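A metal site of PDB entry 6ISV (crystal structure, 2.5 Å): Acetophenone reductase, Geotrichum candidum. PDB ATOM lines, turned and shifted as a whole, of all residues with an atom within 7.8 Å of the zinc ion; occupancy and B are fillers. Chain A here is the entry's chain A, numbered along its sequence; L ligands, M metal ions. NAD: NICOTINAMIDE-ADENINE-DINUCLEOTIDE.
N of Ser 47 sits at hydrogen-bond distance from O2D of the ligand (3.2 Å).
The side-chain hydroxyl of Ser 47 lies within hydrogen-bond range of an oxygen (O2D) of the ligand, 2.8 Å away.
The guanidinium group (NH2) of Arg 333 lies within salt-bridge range of an oxygen (O1N) of the ligand.
The backbone NH (N) of His 46 sits at hydrogen-bond distance from an oxygen (O1N) of the ligand (3.4 Å).
O1A of the ligand is in hydrogen-bond range of ND1 of His 46 (3.1 Å).
N of Leu 184 is in hydrogen-bond range of O2N of the ligand.
An oxygen (O3D) of the ligand is in hydrogen-bond range of the backbone NH (N) of Leu 264, at 2.7 Å.
The side-chain hydroxyl (OG1) of Thr 160 sits at hydrogen-bond distance from the side-chain carboxylate (OD1) of Asp 156 (2.9 Å).
The side-chain hydroxyl of Ser 47 lies close to the side-chain sulfur of Cys 45 (3.2 Å).
NH2 of Arg 333 sits close to SG of Cys 45 (3.1 Å).
Ser 47 touches the zinc ion.
Of the 20 residues printed, 4 come within 4 Å of the zinc ion.
The nearest printed residue that does not touch the zinc ion is Arg 333 (4.8 Å).
NE2 of His 66 binds the zinc ion (2.1 Å).
OD2 of Asp 156 is bound to the zinc ion (2.1 Å).
The side-chain sulfur (SG) of Cys 45 binds the zinc ion (2.4 Å).
The zinc ion has three donor atoms within binding distance.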
ATOM      1  N   GLY A  43      25.766  -6.451 -14.747  1.00  0.00           N
ATOM      2  CA  GLY A  43      25.890  -5.954 -16.097  1.00  0.00           C
ATOM      3  C   GLY A  43      27.268  -5.369 -16.375  1.00  0.00           C
ATOM      4  O   GLY A  43      27.944  -4.830 -15.510  1.00  0.00           O
ATOM      5  N   VAL A  44      27.676  -5.473 -17.641  1.00  0.00           N
ATOM      6  CA  VAL A  44      28.986  -5.032 -18.084  1.00  0.00           C
ATOM      7  C   VAL A  44      28.808  -3.770 -18.910  1.00  0.00           C
ATOM      8  O   VAL A  44      28.190  -3.799 -19.984  1.00  0.00           O
ATOM      9  CB  VAL A  44      29.693  -6.135 -18.895  1.00  0.00           C
ATOM     10  CG1 VAL A  44      31.059  -5.693 -19.287  1.00  0.00           C
ATOM     11  CG2 VAL A  44      29.769  -7.416 -18.083  1.00  0.00           C
ATOM     12  N   CYS A  45      29.361  -2.663 -18.427  1.00  0.00           N
ATOM     13  CA  CYS A  45      29.194  -1.331 -18.997  1.00  0.00           C
ATOM     14  C   CYS A  45      30.492  -0.827 -19.625  1.00  0.00           C
ATOM     15  O   CYS A  45      31.577  -1.031 -19.069  1.00  0.00           O
ATOM     16  CB  CYS A  45      28.740  -0.330 -17.934  1.00  0.00           C
ATOM     17  SG  CYS A  45      28.370   1.298 -18.562  1.00  0.00           S
ATOM     18  N   HIS A  46      30.373  -0.146 -20.774  1.00  0.00           N
ATOM     19  CA  HIS A  46      31.545   0.336 -21.524  1.00  0.00           C
ATOM     20  C   HIS A  46      32.346   1.326 -20.701  1.00  0.00           C
ATOM     21  O   HIS A  46      33.577   1.415 -20.847  1.00  0.00           O
ATOM     22  CB  HIS A  46      31.104   0.958 -22.860  1.00  0.00           C
ATOM     23  CG  HIS A  46      32.203   1.081 -23.880  1.00  0.00           C
ATOM     24  ND1 HIS A  46      32.062   0.665 -25.192  1.00  0.00           N
ATOM     25  CD2 HIS A  46      33.446   1.619 -23.795  1.00  0.00           C
ATOM     26  CE1 HIS A  46      33.176   0.916 -25.848  1.00  0.00           C
ATOM     27  NE2 HIS A  46      34.031   1.494 -25.031  1.00  0.00           N
ATOM     28  N   SER A  47      31.670   2.081 -19.825  1.00  0.00           N
ATOM     29  CA  SER A  47      32.400   2.917 -18.867  1.00  0.00           C
ATOM     30  C   SER A  47      33.509   2.158 -18.167  1.00  0.00           C
ATOM     31  O   SER A  47      34.501   2.757 -17.746  1.00  0.00           O
ATOM     32  CB  SER A  47      31.441   3.485 -17.822  1.00  0.00           C
ATOM     33  OG  SER A  47      30.232   3.892 -18.411  1.00  0.00           O
ATOM     34  N   ASP A  48      33.373   0.826 -18.039  1.00  0.00           N
ATOM     35  CA  ASP A  48      34.412   0.050 -17.381  1.00  0.00           C
ATOM     36  C   ASP A  48      35.643  -0.074 -18.279  1.00  0.00           C
ATOM     37  O   ASP A  48      36.773  -0.070 -17.779  1.00  0.00           O
ATOM     38  CB  ASP A  48      33.865  -1.331 -16.975  1.00  0.00           C
ATOM     39  CG  ASP A  48      32.827  -1.251 -15.832  1.00  0.00           C
ATOM     40  OD1 ASP A  48      32.994  -0.397 -14.920  1.00  0.00           O
ATOM     41  OD2 ASP A  48      31.836  -2.025 -15.835  1.00  0.00           O
ATOM     42  N   LEU A  64      34.635  -3.012  -9.829  1.00  0.00           N
ATOM     43  CA  LEU A  64      34.197  -2.044 -10.824  1.00  0.00           C
ATOM     44  C   LEU A  64      32.777  -2.231 -11.371  1.00  0.00           C
ATOM     45  O   LEU A  64      32.318  -1.371 -12.142  1.00  0.00           O
ATOM     46  CB  LEU A  64      35.168  -2.039 -12.014  1.00  0.00           C
ATOM     47  CG  LEU A  64      36.492  -1.263 -11.873  1.00  0.00           C
ATOM     48  CD1 LEU A  64      37.032  -0.920 -13.231  1.00  0.00           C
ATOM     49  CD2 LEU A  64      36.323  -0.004 -11.049  1.00  0.00           C
ATOM     50  N   HIS A  66      28.790  -2.055 -11.835  1.00  0.00           N
ATOM     51  CA  HIS A  66      27.811  -1.119 -11.299  1.00  0.00           C
ATOM     52  C   HIS A  66      26.414  -1.350 -11.840  1.00  0.00           C
ATOM     53  O   HIS A  66      25.543  -0.489 -11.634  1.00  0.00           O
ATOM     54  CB  HIS A  66      28.229   0.338 -11.560  1.00  0.00           C
ATOM     55  CG  HIS A  66      28.422   0.677 -13.012  1.00  0.00           C
ATOM     56  ND1 HIS A  66      29.606   0.436 -13.672  1.00  0.00           N
ATOM     57  CD2 HIS A  66      27.596   1.251 -13.906  1.00  0.00           C
ATOM     58  CE1 HIS A  66      29.491   0.848 -14.921  1.00  0.00           C
ATOM     59  NE2 HIS A  66      28.278   1.348 -15.092  1.00  0.00           N
ATOM     60  N   GLU A  67      26.160  -2.467 -12.527  1.00  0.00           N
ATOM     61  CA  GLU A  67      24.806  -2.888 -12.870  1.00  0.00           C
ATOM     62  C   GLU A  67      24.470  -4.097 -11.992  1.00  0.00           C
ATOM     63  O   GLU A  67      24.704  -5.228 -12.380  1.00  0.00           O
ATOM     64  CB  GLU A  67      24.702  -3.195 -14.363  1.00  0.00           C
ATOM     65  CG  GLU A  67      24.569  -1.963 -15.256  1.00  0.00           C
ATOM     66  CD  GLU A  67      24.446  -2.280 -16.755  1.00  0.00           C
ATOM     67  OE1 GLU A  67      23.644  -1.615 -17.445  1.00  0.00           O
ATOM     68  OE2 GLU A  67      25.156  -3.167 -17.269  1.00  0.00           O
ATOM     69  N   TYR A 120      28.544   3.202  -7.085  1.00  0.00           N
ATOM     70  CA  TYR A 120      29.036   1.832  -7.248  1.00  0.00           C
ATOM     71  C   TYR A 120      30.105   1.788  -8.323  1.00  0.00           C
ATOM     72  O   TYR A 120      30.042   2.489  -9.344  1.00  0.00           O
ATOM     73  CB  TYR A 120      27.883   0.890  -7.623  1.00  0.00           C
ATOM     74  CG  TYR A 120      27.086   0.339  -6.457  1.00  0.00           C
ATOM     75  CD1 TYR A 120      27.528  -0.760  -5.740  1.00  0.00           C
ATOM     76  CD2 TYR A 120      25.878   0.918  -6.082  1.00  0.00           C
ATOM     77  CE1 TYR A 120      26.788  -1.271  -4.676  1.00  0.00           C
ATOM     78  CE2 TYR A 120      25.136   0.426  -5.027  1.00  0.00           C
ATOM     79  CZ  TYR A 120      25.598  -0.666  -4.331  1.00  0.00           C
ATOM     80  OH  TYR A 120      24.883  -1.164  -3.268  1.00  0.00           O
ATOM     81  N   LEU A 122      32.864   2.947  -8.879  1.00  0.00           N
ATOM     82  CA  LEU A 122      33.810   4.045  -8.988  1.00  0.00           C
ATOM     83  C   LEU A 122      34.401   4.320  -7.621  1.00  0.00           C
ATOM     84  O   LEU A 122      34.638   5.471  -7.243  1.00  0.00           O
ATOM     85  CB  LEU A 122      33.172   5.308  -9.579  1.00  0.00           C
ATOM     86  CG  LEU A 122      32.009   5.172 -10.586  1.00  0.00           C
ATOM     87  CD1 LEU A 122      31.370   6.525 -10.994  1.00  0.00           C
ATOM     88  CD2 LEU A 122      32.422   4.388 -11.837  1.00  0.00           C
ATOM     89  N   THR A 155      19.160  -0.798 -14.483  1.00  0.00           N
ATOM     90  CA  THR A 155      19.676   0.257 -13.619  1.00  0.00           C
ATOM     91  C   THR A 155      20.660   1.204 -14.302  1.00  0.00           C
ATOM     92  O   THR A 155      20.981   2.241 -13.718  1.00  0.00           O
ATOM     93  CB  THR A 155      20.399  -0.318 -12.401  1.00  0.00           C
ATOM     94  OG1 THR A 155      21.761  -0.616 -12.765  1.00  0.00           O
ATOM     95  CG2 THR A 155      19.682  -1.554 -11.865  1.00  0.00           C
ATOM     96  N   ASP A 156      21.171   0.879 -15.491  1.00  0.00           N
ATOM     97  CA  ASP A 156      22.122   1.781 -16.135  1.00  0.00           C
ATOM     98  C   ASP A 156      21.804   1.908 -17.622  1.00  0.00           C
ATOM     99  O   ASP A 156      21.313   2.959 -18.065  1.00  0.00           O
ATOM    100  CB  ASP A 156      23.551   1.264 -15.884  1.00  0.00           C
ATOM    101  CG  ASP A 156      24.640   2.093 -16.580  1.00  0.00           C
ATOM    102  OD1 ASP A 156      24.382   3.268 -16.952  1.00  0.00           O
ATOM    103  OD2 ASP A 156      25.761   1.540 -16.761  1.00  0.00           O
ATOM    104  N   ALA A 157      22.046   0.839 -18.371  1.00  0.00           N
ATOM    105  CA  ALA A 157      21.812   0.843 -19.822  1.00  0.00           C
ATOM    106  C   ALA A 157      20.399   1.276 -20.198  1.00  0.00           C
ATOM    107  O   ALA A 157      20.198   1.822 -21.285  1.00  0.00           O
ATOM    108  CB  ALA A 157      22.114  -0.544 -20.387  1.00  0.00           C
ATOM    109  N   THR A 160      20.010   5.311 -17.671  1.00  0.00           N
ATOM    110  CA  THR A 160      20.739   6.498 -18.102  1.00  0.00           C
ATOM    111  C   THR A 160      20.110   7.152 -19.333  1.00  0.00           C
ATOM    112  O   THR A 160      19.847   8.374 -19.290  1.00  0.00           O
ATOM    113  CB  THR A 160      22.216   6.147 -18.351  1.00  0.00           C
ATOM    114  OG1 THR A 160      22.837   5.667 -17.139  1.00  0.00           O
ATOM    115  CG2 THR A 160      22.965   7.367 -18.877  1.00  0.00           C
ATOM    116  N   LEU A 184      23.382   0.909 -24.152  1.00  0.00           N
ATOM    117  CA  LEU A 184      22.556   2.095 -23.950  1.00  0.00           C
ATOM    118  C   LEU A 184      21.694   2.376 -25.170  1.00  0.00           C
ATOM    119  O   LEU A 184      20.483   2.598 -25.042  1.00  0.00           O
ATOM    120  CB  LEU A 184      23.431   3.311 -23.612  1.00  0.00           C
ATOM    121  CG  LEU A 184      23.710   3.535 -22.126  1.00  0.00           C
ATOM    122  CD1 LEU A 184      24.537   2.383 -21.578  1.00  0.00           C
ATOM    123  CD2 LEU A 184      24.429   4.854 -21.881  1.00  0.00           C
ATOM    124  N   LEU A 264      31.052   8.558 -23.042  1.00  0.00           N
ATOM    125  CA  LEU A 264      32.364   8.945 -22.527  1.00  0.00           C
ATOM    126  C   LEU A 264      33.468   8.547 -23.507  1.00  0.00           C
ATOM    127  O   LEU A 264      34.588   8.232 -23.094  1.00  0.00           O
ATOM    128  CB  LEU A 264      32.629   8.330 -21.154  1.00  0.00           C
ATOM    129  CG  LEU A 264      31.813   8.872 -19.974  1.00  0.00           C
ATOM    130  CD1 LEU A 264      31.944   7.996 -18.727  1.00  0.00           C
ATOM    131  CD2 LEU A 264      32.229  10.295 -19.663  1.00  0.00           C
ATOM    132  N   PHE A 287      23.721  12.283 -16.282  1.00  0.00           N
ATOM    133  CA  PHE A 287      24.535  11.277 -15.585  1.00  0.00           C
ATOM    134  C   PHE A 287      23.658  10.278 -14.837  1.00  0.00           C
ATOM    135  O   PHE A 287      22.907  10.674 -13.939  1.00  0.00           O
ATOM    136  CB  PHE A 287      25.479  11.984 -14.616  1.00  0.00           C
ATOM    137  CG  PHE A 287      26.308  11.049 -13.755  1.00  0.00           C
ATOM    138  CD1 PHE A 287      27.219  10.168 -14.306  1.00  0.00           C
ATOM    139  CD2 PHE A 287      26.190  11.098 -12.370  1.00  0.00           C
ATOM    140  CE1 PHE A 287      27.984   9.329 -13.501  1.00  0.00           C
ATOM    141  CE2 PHE A 287      26.959  10.284 -11.566  1.00  0.00           C
ATOM    142  CZ  PHE A 287      27.851   9.392 -12.124  1.00  0.00           C
ATOM    143  N   TRP A 288      23.798   8.975 -15.145  1.00  0.00           N
ATOM    144  CA  TRP A 288      23.072   7.873 -14.475  1.00  0.00           C
ATOM    145  C   TRP A 288      21.559   8.171 -14.527  1.00  0.00           C
ATOM    146  O   TRP A 288      21.054   8.666 -15.531  1.00  0.00           O
ATOM    147  CB  TRP A 288      23.513   7.704 -13.015  1.00  0.00           C
ATOM    148  CG  TRP A 288      24.556   6.636 -12.562  1.00  0.00           C
ATOM    149  CD1 TRP A 288      25.776   6.881 -11.913  1.00  0.00           C
ATOM    150  CD2 TRP A 288      24.436   5.203 -12.593  1.00  0.00           C
ATOM    151  NE1 TRP A 288      26.421   5.703 -11.580  1.00  0.00           N
ATOM    152  CE2 TRP A 288      25.628   4.655 -11.984  1.00  0.00           C
ATOM    153  CE3 TRP A 288      23.468   4.327 -13.084  1.00  0.00           C
ATOM    154  CZ2 TRP A 288      25.863   3.290 -11.877  1.00  0.00           C
ATOM    155  CZ3 TRP A 288      23.702   2.966 -12.949  1.00  0.00           C
ATOM    156  CH2 TRP A 288      24.880   2.463 -12.366  1.00  0.00           C
ATOM    157  N   ARG A 333      24.137  -5.661 -24.768  1.00  0.00           N
ATOM    158  CA  ARG A 333      24.735  -5.691 -23.454  1.00  0.00           C
ATOM    159  C   ARG A 333      24.890  -7.131 -22.986  1.00  0.00           C
ATOM    160  O   ARG A 333      24.033  -7.980 -23.242  1.00  0.00           O
ATOM    161  CB  ARG A 333      23.913  -4.889 -22.430  1.00  0.00           C
ATOM    162  CG  ARG A 333      24.810  -4.430 -21.279  1.00  0.00           C
ATOM    163  CD  ARG A 333      24.203  -3.370 -20.489  1.00  0.00           C
ATOM    164  NE  ARG A 333      25.137  -2.395 -19.967  1.00  0.00           N
ATOM    165  CZ  ARG A 333      25.584  -1.370 -20.680  1.00  0.00           C
ATOM    166  NH1 ARG A 333      25.181  -1.236 -21.936  1.00  0.00           N
ATOM    167  NH2 ARG A 333      26.410  -0.493 -20.151  1.00  0.00           N
HETATM  168  PA  NAD L   1      28.472  -0.669 -26.035  1.00  0.00           P
HETATM  169  O1A NAD L   1      29.820  -1.277 -26.112  1.00  0.00           O
HETATM  170  O2A NAD L   1      27.342  -1.488 -25.555  1.00  0.00           O
HETATM  171  O5B NAD L   1      28.087  -0.135 -27.503  1.00  0.00           O
HETATM  172  C5B NAD L   1      28.494   1.159 -27.954  1.00  0.00           C
HETATM  173  C4B NAD L   1      28.102   1.339 -29.434  1.00  0.00           C
HETATM  174  O4B NAD L   1      28.841   2.503 -29.919  1.00  0.00           O
HETATM  175  C3B NAD L   1      28.555   0.158 -30.308  1.00  0.00           C
HETATM  176  O3B NAD L   1      27.463  -0.352 -31.082  1.00  0.00           O
HETATM  177  C2B NAD L   1      29.513   0.873 -31.231  1.00  0.00           C
HETATM  178  O2B NAD L   1      29.478   0.275 -32.535  1.00  0.00           O
HETATM  179  C1B NAD L   1      28.914   2.242 -31.291  1.00  0.00           C
HETATM  180  N9A NAD L   1      29.883   3.207 -31.855  1.00  0.00           N
HETATM  181  C8A NAD L   1      31.140   3.366 -31.424  1.00  0.00           C
HETATM  182  N7A NAD L   1      31.706   4.326 -32.148  1.00  0.00           N
HETATM  183  C5A NAD L   1      30.807   4.761 -33.044  1.00  0.00           C
HETATM  184  C6A NAD L   1      30.882   5.698 -33.986  1.00  0.00           C
HETATM  185  N6A NAD L   1      32.039   6.336 -34.113  1.00  0.00           N
HETATM  186  N1A NAD L   1      29.843   5.974 -34.784  1.00  0.00           N
HETATM  187  C2A NAD L   1      28.646   5.275 -34.616  1.00  0.00           C
HETATM  188  N3A NAD L   1      28.596   4.291 -33.612  1.00  0.00           N
HETATM  189  C4A NAD L   1      29.680   4.066 -32.854  1.00  0.00           C
HETATM  190  O3  NAD L   1      28.592   0.727 -25.182  1.00  0.00           O
HETATM  191  PN  NAD L   1      27.526   1.196 -24.044  1.00  0.00           P
HETATM  192  O1N NAD L   1      27.724   0.361 -22.821  1.00  0.00           O
HETATM  193  O2N NAD L   1      26.194   1.326 -24.657  1.00  0.00           O
HETATM  194  O5D NAD L   1      28.026   2.676 -23.694  1.00  0.00           O
HETATM  195  C5D NAD L   1      28.247   3.667 -24.695  1.00  0.00           C
HETATM  196  C4D NAD L   1      28.766   4.947 -24.031  1.00  0.00           C
HETATM  197  O4D NAD L   1      27.845   5.282 -22.933  1.00  0.00           O
HETATM  198  C3D NAD L   1      30.117   4.736 -23.331  1.00  0.00           C
HETATM  199  O3D NAD L   1      30.921   5.912 -23.502  1.00  0.00           O
HETATM  200  C2D NAD L   1      29.643   4.648 -21.884  1.00  0.00           C
HETATM  201  O2D NAD L   1      30.721   4.887 -20.976  1.00  0.00           O
HETATM  202  C1D NAD L   1      28.654   5.755 -21.857  1.00  0.00           C
HETATM  203  N1N NAD L   1      27.823   5.806 -20.591  1.00  0.00           N
HETATM  204  C2N NAD L   1      27.355   7.048 -20.086  1.00  0.00           C
HETATM  205  C3N NAD L   1      26.573   7.121 -18.935  1.00  0.00           C
HETATM  206  C7N NAD L   1      26.142   8.367 -18.452  1.00  0.00           C
HETATM  207  O7N NAD L   1      25.947   9.316 -19.203  1.00  0.00           O
HETATM  208  N7N NAD L   1      25.940   8.422 -17.140  1.00  0.00           N
HETATM  209  C4N NAD L   1      26.246   5.947 -18.274  1.00  0.00           C
HETATM  210  C5N NAD L   1      26.678   4.713 -18.752  1.00  0.00           C
HETATM  211  C6N NAD L   1      27.459   4.627 -19.909  1.00  0.00           C
HETATM  212 ZN    ZN M   1      27.636   2.570 -16.688  1.00  0.00          ZN
